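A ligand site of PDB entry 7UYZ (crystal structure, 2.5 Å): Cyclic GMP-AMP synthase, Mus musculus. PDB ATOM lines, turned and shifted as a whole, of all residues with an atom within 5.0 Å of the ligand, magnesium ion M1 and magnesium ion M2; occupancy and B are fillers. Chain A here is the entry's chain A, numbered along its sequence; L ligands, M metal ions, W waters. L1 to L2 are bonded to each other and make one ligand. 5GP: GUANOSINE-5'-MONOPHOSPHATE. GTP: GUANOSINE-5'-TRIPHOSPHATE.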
ATOM      1  N   GLY A  55       8.079  11.229   1.543  1.00  0.00           N
ATOM      2  CA  GLY A  55       8.037   9.774   1.534  1.00  0.00           C
ATOM      3  C   GLY A  55       9.389   9.142   1.813  1.00  0.00           C
ATOM      4  O   GLY A  55      10.370   9.838   2.095  1.00  0.00           O
ATOM      5  N   SER A  56       9.419   7.806   1.678  1.00  0.00           N
ATOM      6  CA  SER A  56      10.538   6.947   2.035  1.00  0.00           C
ATOM      7  C   SER A  56      11.871   7.430   1.552  1.00  0.00           C
ATOM      8  O   SER A  56      12.841   7.443   2.309  1.00  0.00           O
ATOM      9  CB  SER A  56      10.379   5.566   1.412  1.00  0.00           C
ATOM     10  OG  SER A  56       9.170   5.010   1.791  1.00  0.00           O
ATOM     11  N   GLU A  59      13.049  10.399   3.159  1.00  0.00           N
ATOM     12  CA  GLU A  59      13.206  10.065   4.578  1.00  0.00           C
ATOM     13  C   GLU A  59      14.374   9.089   4.886  1.00  0.00           C
ATOM     14  O   GLU A  59      14.657   8.817   6.045  1.00  0.00           O
ATOM     15  CB  GLU A  59      11.904   9.486   5.114  1.00  0.00           C
ATOM     16  CG  GLU A  59      10.789  10.513   5.304  1.00  0.00           C
ATOM     17  CD  GLU A  59       9.424   9.854   5.491  1.00  0.00           C
ATOM     18  OE1 GLU A  59       9.348   8.606   5.380  1.00  0.00           O
ATOM     19  OE2 GLU A  59       8.440  10.578   5.754  1.00  0.00           O
ATOM     20  N   LYS A  62      13.578   4.186   2.258  1.00  0.00           N
ATOM     21  CA  LYS A  62      13.221   3.419   1.067  1.00  0.00           C
ATOM     22  C   LYS A  62      14.056   2.157   1.093  1.00  0.00           C
ATOM     23  O   LYS A  62      15.242   2.205   1.354  1.00  0.00           O
ATOM     24  CB  LYS A  62      13.482   4.214  -0.204  1.00  0.00           C
ATOM     25  CG  LYS A  62      13.005   3.514  -1.490  1.00  0.00           C
ATOM     26  CD  LYS A  62      11.486   3.547  -1.621  1.00  0.00           C
ATOM     27  CE  LYS A  62      11.010   2.787  -2.851  1.00  0.00           C
ATOM     28  NZ  LYS A  62      11.431   1.378  -2.895  1.00  0.00           N
ATOM     29  N   GLU A  68      10.427   4.066  -6.252  1.00  0.00           N
ATOM     30  CA  GLU A  68       9.210   4.777  -5.946  1.00  0.00           C
ATOM     31  C   GLU A  68       9.579   6.065  -5.230  1.00  0.00           C
ATOM     32  O   GLU A  68      10.326   6.056  -4.254  1.00  0.00           O
ATOM     33  CB  GLU A  68       8.244   3.886  -5.158  1.00  0.00           C
ATOM     34  CG  GLU A  68       6.762   4.231  -5.327  1.00  0.00           C
ATOM     35  CD  GLU A  68       6.246   5.243  -4.303  1.00  0.00           C
ATOM     36  OE1 GLU A  68       7.042   5.660  -3.444  1.00  0.00           O
ATOM     37  OE2 GLU A  68       5.048   5.617  -4.342  1.00  0.00           O
ATOM     38  N   ASP A  70       7.971  10.091  -4.111  1.00  0.00           N
ATOM     39  CA  ASP A  70       6.780  10.883  -3.850  1.00  0.00           C
ATOM     40  C   ASP A  70       7.128  12.368  -3.820  1.00  0.00           C
ATOM     41  O   ASP A  70       8.068  12.778  -3.123  1.00  0.00           O
ATOM     42  CB  ASP A  70       6.118  10.419  -2.555  1.00  0.00           C
ATOM     43  CG  ASP A  70       5.940   8.905  -2.530  1.00  0.00           C
ATOM     44  OD1 ASP A  70       4.964   8.388  -3.146  1.00  0.00           O
ATOM     45  OD2 ASP A  70       6.801   8.241  -1.915  1.00  0.00           O
ATOM     46  N   GLU A 142       0.275   6.532 -15.476  1.00  0.00           N
ATOM     47  CA  GLU A 142      -0.470   5.346 -15.093  1.00  0.00           C
ATOM     48  C   GLU A 142      -1.950   5.695 -15.112  1.00  0.00           C
ATOM     49  O   GLU A 142      -2.337   6.821 -14.853  1.00  0.00           O
ATOM     50  CB  GLU A 142      -0.031   4.883 -13.700  1.00  0.00           C
ATOM     51  CG  GLU A 142      -0.488   3.509 -13.230  1.00  0.00           C
ATOM     52  CD  GLU A 142      -0.186   3.284 -11.724  1.00  0.00           C
ATOM     53  OE1 GLU A 142      -0.892   3.868 -10.870  1.00  0.00           O
ATOM     54  OE2 GLU A 142       0.786   2.577 -11.382  1.00  0.00           O
ATOM     55  N   LYS A 145      -6.089   5.387 -10.503  1.00  0.00           N
ATOM     56  CA  LYS A 145      -6.606   4.480  -9.514  1.00  0.00           C
ATOM     57  C   LYS A 145      -7.543   5.279  -8.610  1.00  0.00           C
ATOM     58  O   LYS A 145      -7.144   6.317  -8.096  1.00  0.00           O
ATOM     59  CB  LYS A 145      -5.476   3.890  -8.690  1.00  0.00           C
ATOM     60  CG  LYS A 145      -4.661   2.916  -9.506  1.00  0.00           C
ATOM     61  CD  LYS A 145      -3.607   2.232  -8.660  1.00  0.00           C
ATOM     62  CE  LYS A 145      -2.888   1.182  -9.503  1.00  0.00           C
ATOM     63  NZ  LYS A 145      -2.125   0.235  -8.639  1.00  0.00           N
ATOM     64  N   GLY A 147      -9.541   6.464  -5.284  1.00  0.00           N
ATOM     65  CA  GLY A 147      -9.028   6.593  -3.939  1.00  0.00           C
ATOM     66  C   GLY A 147      -7.664   7.223  -3.877  1.00  0.00           C
ATOM     67  O   GLY A 147      -7.142   7.392  -2.774  1.00  0.00           O
ATOM     68  N   SER A 148      -7.064   7.578  -5.024  1.00  0.00           N
ATOM     69  CA  SER A 148      -5.725   8.153  -5.052  1.00  0.00           C
ATOM     70  C   SER A 148      -5.664   9.645  -5.408  1.00  0.00           C
ATOM     71  O   SER A 148      -6.234  10.075  -6.391  1.00  0.00           O
ATOM     72  CB  SER A 148      -4.805   7.372  -5.977  1.00  0.00           C
ATOM     73  OG  SER A 148      -3.486   7.901  -5.897  1.00  0.00           O
ATOM     74  N   ASP A 164       4.813   9.350  -7.780  1.00  0.00           N
ATOM     75  CA  ASP A 164       3.520   9.899  -7.432  1.00  0.00           C
ATOM     76  C   ASP A 164       3.691  11.418  -7.407  1.00  0.00           C
ATOM     77  O   ASP A 164       4.465  11.941  -6.596  1.00  0.00           O
ATOM     78  CB  ASP A 164       3.069   9.417  -6.044  1.00  0.00           C
ATOM     79  CG  ASP A 164       2.750   7.930  -5.998  1.00  0.00           C
ATOM     80  OD1 ASP A 164       2.376   7.353  -7.038  1.00  0.00           O
ATOM     81  OD2 ASP A 164       2.898   7.331  -4.899  1.00  0.00           O
ATOM     82  N   ARG A 221      -8.464  15.550   1.877  1.00  0.00           N
ATOM     83  CA  ARG A 221      -7.885  14.852   3.071  1.00  0.00           C
ATOM     84  C   ARG A 221      -6.609  15.586   3.518  1.00  0.00           C
ATOM     85  O   ARG A 221      -5.834  15.996   2.625  1.00  0.00           O
ATOM     86  CB  ARG A 221      -7.584  13.381   2.776  1.00  0.00           C
ATOM     87  CG  ARG A 221      -6.995  12.605   3.962  1.00  0.00           C
ATOM     88  CD  ARG A 221      -6.680  11.153   3.651  1.00  0.00           C
ATOM     89  NE  ARG A 221      -5.358  10.948   3.040  1.00  0.00           N
ATOM     90  CZ  ARG A 221      -5.124  10.511   1.788  1.00  0.00           C
ATOM     91  NH1 ARG A 221      -6.114  10.239   0.941  1.00  0.00           N
ATOM     92  NH2 ARG A 221      -3.866  10.342   1.382  1.00  0.00           N
ATOM     93  N   SER A 225       2.877  14.960   5.524  1.00  0.00           N
ATOM     94  CA  SER A 225       4.081  14.376   5.000  1.00  0.00           C
ATOM     95  C   SER A 225       5.316  15.200   5.260  1.00  0.00           C
ATOM     96  O   SER A 225       6.405  14.647   5.393  1.00  0.00           O
ATOM     97  CB  SER A 225       3.981  14.208   3.497  1.00  0.00           C
ATOM     98  OG  SER A 225       3.033  13.235   3.204  1.00  0.00           O
ATOM     99  N   LYS A 259       8.481  -2.567   7.253  1.00  0.00           N
ATOM    100  CA  LYS A 259       8.087  -2.218   5.905  1.00  0.00           C
ATOM    101  C   LYS A 259       8.299  -3.387   4.952  1.00  0.00           C
ATOM    102  O   LYS A 259       7.450  -3.651   4.091  1.00  0.00           O
ATOM    103  CB  LYS A 259       8.910  -1.015   5.394  1.00  0.00           C
ATOM    104  CG  LYS A 259       8.316   0.325   5.737  1.00  0.00           C
ATOM    105  CD  LYS A 259       9.364   1.415   5.645  1.00  0.00           C
ATOM    106  CE  LYS A 259       9.714   1.748   4.201  1.00  0.00           C
ATOM    107  NZ  LYS A 259       8.561   2.337   3.456  1.00  0.00           N
ATOM    108  N   GLU A 263       5.575  -5.510   2.722  1.00  0.00           N
ATOM    109  CA  GLU A 263       5.806  -5.582   1.267  1.00  0.00           C
ATOM    110  C   GLU A 263       5.883  -7.027   0.758  1.00  0.00           C
ATOM    111  O   GLU A 263       5.309  -7.372  -0.299  1.00  0.00           O
ATOM    112  CB  GLU A 263       7.097  -4.842   0.867  1.00  0.00           C
ATOM    113  CG  GLU A 263       6.977  -3.332   0.741  1.00  0.00           C
ATOM    114  CD  GLU A 263       8.210  -2.668   0.155  1.00  0.00           C
ATOM    115  OE1 GLU A 263       8.869  -3.309  -0.695  1.00  0.00           O
ATOM    116  OE2 GLU A 263       8.531  -1.508   0.527  1.00  0.00           O
ATOM    117  N   LYS A 266       2.490  -8.693   1.140  1.00  0.00           N
ATOM    118  CA  LYS A 266       1.557  -8.054   0.219  1.00  0.00           C
ATOM    119  C   LYS A 266       1.744  -8.565  -1.205  1.00  0.00           C
ATOM    120  O   LYS A 266       0.770  -8.748  -1.941  1.00  0.00           O
ATOM    121  CB  LYS A 266       1.733  -6.527   0.209  1.00  0.00           C
ATOM    122  CG  LYS A 266       1.391  -5.798   1.499  1.00  0.00           C
ATOM    123  CD  LYS A 266       0.154  -4.950   1.409  1.00  0.00           C
ATOM    124  CE  LYS A 266       0.285  -3.766   0.443  1.00  0.00           C
ATOM    125  NZ  LYS A 266      -1.062  -3.643  -0.158  1.00  0.00           N
ATOM    126  N   PHE A 275      -4.060  -3.158   3.341  1.00  0.00           N
ATOM    127  CA  PHE A 275      -2.945  -2.681   4.115  1.00  0.00           C
ATOM    128  C   PHE A 275      -1.910  -1.946   3.277  1.00  0.00           C
ATOM    129  O   PHE A 275      -1.799  -2.176   2.087  1.00  0.00           O
ATOM    130  CB  PHE A 275      -2.292  -3.851   4.825  1.00  0.00           C
ATOM    131  CG  PHE A 275      -3.196  -4.532   5.771  1.00  0.00           C
ATOM    132  CD1 PHE A 275      -3.474  -3.945   6.999  1.00  0.00           C
ATOM    133  CD2 PHE A 275      -3.796  -5.725   5.439  1.00  0.00           C
ATOM    134  CE1 PHE A 275      -4.340  -4.556   7.885  1.00  0.00           C
ATOM    135  CE2 PHE A 275      -4.671  -6.345   6.319  1.00  0.00           C
ATOM    136  CZ  PHE A 275      -4.928  -5.753   7.559  1.00  0.00           C
ATOM    137  N   CYS A 276      -1.147  -1.056   3.920  1.00  0.00           N
ATOM    138  CA  CYS A 276      -0.190  -0.214   3.232  1.00  0.00           C
ATOM    139  C   CYS A 276       0.898   0.199   4.199  1.00  0.00           C
ATOM    140  O   CYS A 276       0.703   0.127   5.395  1.00  0.00           O
ATOM    141  CB  CYS A 276      -0.870   1.018   2.652  1.00  0.00           C
ATOM    142  SG  CYS A 276      -1.466   2.201   3.875  1.00  0.00           S
ATOM    143  N   SER A 277       2.025   0.657   3.665  1.00  0.00           N
ATOM    144  CA  SER A 277       3.179   1.041   4.462  1.00  0.00           C
ATOM    145  C   SER A 277       2.858   2.142   5.489  1.00  0.00           C
ATOM    146  O   SER A 277       3.525   2.242   6.501  1.00  0.00           O
ATOM    147  CB  SER A 277       4.343   1.475   3.569  1.00  0.00           C
ATOM    148  OG  SER A 277       4.019   2.654   2.850  1.00  0.00           O
ATOM    149  N   TYR A 278       1.856   2.978   5.215  1.00  0.00           N
ATOM    150  CA  TYR A 278       1.496   4.102   6.103  1.00  0.00           C
ATOM    151  C   TYR A 278       0.989   3.539   7.433  1.00  0.00           C
ATOM    152  O   TYR A 278       1.067   4.242   8.458  1.00  0.00           O
ATOM    153  CB  TYR A 278       0.462   5.050   5.470  1.00  0.00           C
ATOM    154  CG  TYR A 278       0.337   6.342   6.252  1.00  0.00           C
ATOM    155  CD1 TYR A 278       1.374   7.267   6.232  1.00  0.00           C
ATOM    156  CD2 TYR A 278      -0.756   6.618   7.071  1.00  0.00           C
ATOM    157  CE1 TYR A 278       1.311   8.431   6.966  1.00  0.00           C
ATOM    158  CE2 TYR A 278      -0.830   7.786   7.813  1.00  0.00           C
ATOM    159  CZ  TYR A 278       0.220   8.693   7.770  1.00  0.00           C
ATOM    160  OH  TYR A 278       0.185   9.858   8.480  1.00  0.00           O
ATOM    161  N   LYS A 281       4.041   2.878   9.403  1.00  0.00           N
ATOM    162  CA  LYS A 281       4.725   4.138   9.714  1.00  0.00           C
ATOM    163  C   LYS A 281       4.035   4.776  10.908  1.00  0.00           C
ATOM    164  O   LYS A 281       4.686   5.285  11.809  1.00  0.00           O
ATOM    165  CB  LYS A 281       4.670   5.088   8.508  1.00  0.00           C
ATOM    166  CG  LYS A 281       5.539   6.323   8.610  1.00  0.00           C
ATOM    167  CD  LYS A 281       5.336   7.247   7.418  1.00  0.00           C
ATOM    168  CE  LYS A 281       6.491   8.216   7.237  1.00  0.00           C
ATOM    169  NZ  LYS A 281       6.115   9.455   6.466  1.00  0.00           N
ATOM    170  N   HIS A 324      -4.567   7.522  13.663  1.00  0.00           N
ATOM    171  CA  HIS A 324      -3.697   8.444  12.941  1.00  0.00           C
ATOM    172  C   HIS A 324      -2.903   9.236  13.986  1.00  0.00           C
ATOM    173  O   HIS A 324      -3.485   9.675  14.971  1.00  0.00           O
ATOM    174  CB  HIS A 324      -4.546   9.367  12.084  1.00  0.00           C
ATOM    175  CG  HIS A 324      -3.795  10.025  10.981  1.00  0.00           C
ATOM    176  ND1 HIS A 324      -2.786  10.943  11.212  1.00  0.00           N
ATOM    177  CD2 HIS A 324      -3.894   9.904   9.641  1.00  0.00           C
ATOM    178  CE1 HIS A 324      -2.310  11.368  10.048  1.00  0.00           C
ATOM    179  NE2 HIS A 324      -2.968  10.749   9.083  1.00  0.00           N
HETATM  180  P   5GP L   1      -3.621   4.130  -1.268  1.00  0.00           P
HETATM  181  O1P 5GP L   1      -4.337   2.926  -0.724  1.00  0.00           O
HETATM  182  O3P 5GP L   1      -4.150   5.502  -0.916  1.00  0.00           O
HETATM  183  O5' 5GP L   1      -3.538   4.095  -2.866  1.00  0.00           O
HETATM  184  C5' 5GP L   1      -3.561   2.834  -3.578  1.00  0.00           C
HETATM  185  C4' 5GP L   1      -2.318   2.724  -4.431  1.00  0.00           C
HETATM  186  O4' 5GP L   1      -1.156   2.640  -3.565  1.00  0.00           O
HETATM  187  C3' 5GP L   1      -2.230   1.491  -5.331  1.00  0.00           C
HETATM  188  O3' 5GP L   1      -1.437   1.745  -6.489  1.00  0.00           O
HETATM  189  C2' 5GP L   1      -1.542   0.493  -4.403  1.00  0.00           C
HETATM  190  O2' 5GP L   1      -0.966  -0.592  -5.098  1.00  0.00           O
HETATM  191  C1' 5GP L   1      -0.503   1.400  -3.756  1.00  0.00           C
HETATM  192  N9  5GP L   1       0.017   0.954  -2.463  1.00  0.00           N
HETATM  193  C8  5GP L   1      -0.603   0.188  -1.500  1.00  0.00           C
HETATM  194  N7  5GP L   1       0.167  -0.043  -0.464  1.00  0.00           N
HETATM  195  C5  5GP L   1       1.354   0.622  -0.755  1.00  0.00           C
HETATM  196  C6  5GP L   1       2.549   0.725  -0.004  1.00  0.00           C
HETATM  197  O6  5GP L   1       2.800   0.249   1.107  1.00  0.00           O
HETATM  198  N1  5GP L   1       3.506   1.493  -0.679  1.00  0.00           N
HETATM  199  C2  5GP L   1       3.339   2.077  -1.918  1.00  0.00           C
HETATM  200  N2  5GP L   1       4.374   2.773  -2.415  1.00  0.00           N
HETATM  201  N3  5GP L   1       2.212   1.968  -2.625  1.00  0.00           N
HETATM  202  C4  5GP L   1       1.274   1.236  -1.981  1.00  0.00           C
HETATM  203  PG  GTP L   2       6.985   3.422   0.572  1.00  0.00           P
HETATM  204  O1G GTP L   2       8.373   2.847   0.734  1.00  0.00           O
HETATM  205  O2G GTP L   2       6.845   4.197  -0.719  1.00  0.00           O
HETATM  206  O3G GTP L   2       5.897   2.405   0.782  1.00  0.00           O
HETATM  207  O3B GTP L   2       6.754   4.513   1.761  1.00  0.00           O
HETATM  208  PB  GTP L   2       6.124   5.978   1.732  1.00  0.00           P
HETATM  209  O1B GTP L   2       6.890   6.820   0.777  1.00  0.00           O
HETATM  210  O2B GTP L   2       5.890   6.462   3.132  1.00  0.00           O
HETATM  211  O3A GTP L   2       4.707   5.644   1.051  1.00  0.00           O
HETATM  212  PA  GTP L   2       3.812   6.199  -0.158  1.00  0.00           P
HETATM  213  O1A GTP L   2       4.581   6.193  -1.450  1.00  0.00           O
HETATM  214  O2A GTP L   2       3.141   7.464   0.256  1.00  0.00           O
HETATM  215  O5' GTP L   2       2.696   5.042  -0.223  1.00  0.00           O
HETATM  216  C5' GTP L   2       1.986   4.562   0.955  1.00  0.00           C
HETATM  217  C4' GTP L   2       0.572   4.235   0.558  1.00  0.00           C
HETATM  218  O4' GTP L   2      -0.253   4.104   1.733  1.00  0.00           O
HETATM  219  C3' GTP L   2      -0.135   5.292  -0.290  1.00  0.00           C
HETATM  220  O3' GTP L   2       0.185   5.146  -1.676  1.00  0.00           O
HETATM  221  C2' GTP L   2      -1.600   4.999   0.006  1.00  0.00           C
HETATM  222  O2' GTP L   2      -2.068   3.981  -0.871  1.00  0.00           O
HETATM  223  C1' GTP L   2      -1.570   4.533   1.457  1.00  0.00           C
HETATM  224  N9  GTP L   2      -1.956   5.575   2.405  1.00  0.00           N
HETATM  225  C8  GTP L   2      -3.106   5.618   3.156  1.00  0.00           C
HETATM  226  N7  GTP L   2      -3.201   6.677   3.914  1.00  0.00           N
HETATM  227  C5  GTP L   2      -2.036   7.394   3.654  1.00  0.00           C
HETATM  228  C6  GTP L   2      -1.575   8.625   4.177  1.00  0.00           C
HETATM  229  O6  GTP L   2      -2.133   9.352   5.019  1.00  0.00           O
HETATM  230  N1  GTP L   2      -0.338   8.988   3.639  1.00  0.00           N
HETATM  231  C2  GTP L   2       0.362   8.250   2.721  1.00  0.00           C
HETATM  232  N2  GTP L   2       1.543   8.748   2.323  1.00  0.00           N
HETATM  233  N3  GTP L   2      -0.066   7.094   2.216  1.00  0.00           N
HETATM  234  C4  GTP L   2      -1.260   6.721   2.729  1.00  0.00           C
HETATM  235 MG    MG M   1       6.909   6.159  -1.350  1.00  0.00          MG
HETATM  236 MG    MG M   2       3.599   6.418  -3.234  1.00  0.00          MG
HETATM  237  O   HOH W   1       6.958  -0.304   2.287  1.00  0.00           O
HETATM  238  O   HOH W   2       4.265   4.854   4.596  1.00  0.00           O
HETATM  239  O   HOH W   3       8.965   6.128  -1.368  1.00  0.00           O
HETATM  240  O   HOH W   4      -1.641   9.485   0.288  1.00  0.00           O
HETATM  241  O   HOH W   5       8.089   6.512   4.707  1.00  0.00           O
HETATM  242  O   HOH W   6      -1.391   7.388  -3.491  1.00  0.00           O
HETATM  243  O   HOH W   7      10.125   1.175   0.121  1.00  0.00           O
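An oxygen (O1B) of GTP L2 sits close to the backbone NH (N) of Ser 56 (2.9 Å).
An oxygen (O3B) of GTP L2 is in hydrogen-bond range of the side-chain hydroxyl of Ser 56 (2.5 Å).
The backbone NH of Ser 277 lies within hydrogen-bond range of an oxygen (O6) of 5GP L1.
The side-chain hydroxyl (OG) of Ser 277 sits at hydrogen-bond distance from an oxygen (O3G) of GTP L2, 2.8 Å away.
The side-chain amino group of Lys 145 lies within hydrogen-bond range of an oxygen (O3') of 5GP L1 (2.7 Å).
O1G of GTP L2 lies within salt-bridge range of NZ of Lys 259 (2.8 Å).
SG of Cys 276 is in hydrogen-bond range of O4' of GTP L2 (3.1 Å).
OG of Ser 56 sits at hydrogen-bond distance from NZ of Lys 259, at 3.2 Å.
O of Ser 56 is in hydrogen-bond range of N of Lys 62, at 3.3 Å.
SG of Cys 276 sits close to N of Tyr 278 (3.7 Å).
OH of Tyr 278 lies close to NE2 of His 324, 3.3 Å away.
NZ of Lys 266 lies within hydrogen-bond range of O of Phe 275, 2.8 Å away.
Gly 55 touches the ligand.
Lys 62 touches the ligand.
O of Gly 147 touches O3P of 5GP L1 (3.997 Å).
NZ of Lys 266 touches N7 of 5GP L1, at 3.8 Å.
Phe 275 touches the ligand.
CE2 of Tyr 278 touches O6 of GTP L2, at 3.5 Å.
Of the 22 residues printed, 13 come within 4 Å of the ligand.
Of the 22 residues printed, 3 come within 4 Å of magnesium ion M2.
Magnesium ion M1 is bound by water W3 (2.1 Å), O2G of GTP L2 (2.1 Å), OE1 of Glu 68 (2.2 Å), OD2 of Asp 70 (2.2 Å), O1B of GTP L2 (2.2 Å) and O1A of GTP L2 (2.3 Å).
Magnesium ion M1 has six donor atoms within binding distance.
Magnesium ion M2 is bound by OE2 of Glu 68 (2.0 Å), OD2 of Asp 164 (2.0 Å), O1A of GTP L2 (2.0 Å) and OD1 of Asp 70 (2.4 Å).
Water W3 bridges the backbone carbonyl oxygen (O) of Glu 68 (3.2 Å) and the side-chain hydroxyl (OG) of Ser 56 (3.4 Å).
Water W7 lies within hydrogen-bond range of an oxygen (O1G) of GTP L2 (2.5 Å), the side-chain carboxylate (OE2) of Glu 263 (3.1 Å) and the side-chain amino group (NZ) of Lys 62 (3.3 Å).
Water W5 lies within hydrogen-bond range of the side-chain carboxylate (OE1) of Glu 59 (2.5 Å), an oxygen (O2B) of GTP L2 (2.7 Å) and the side-chain hydroxyl (OG) of Ser 56 (3.5 Å).
Water W2 lies within hydrogen-bond range of O2B of GTP L2 (2.7 Å), OG of Ser 277 (2.8 Å) and N of Tyr 278 (3.1 Å).
Water W1 lies within hydrogen-bond range of the side-chain carboxylate of Glu 263 (2.6 Å), an oxygen (O3G) of GTP L2 (3.3 Å) and the side-chain amino group of Lys 259 (3.3 Å).
Water W6 bridges OG of Ser 148 and O3' of GTP L2.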
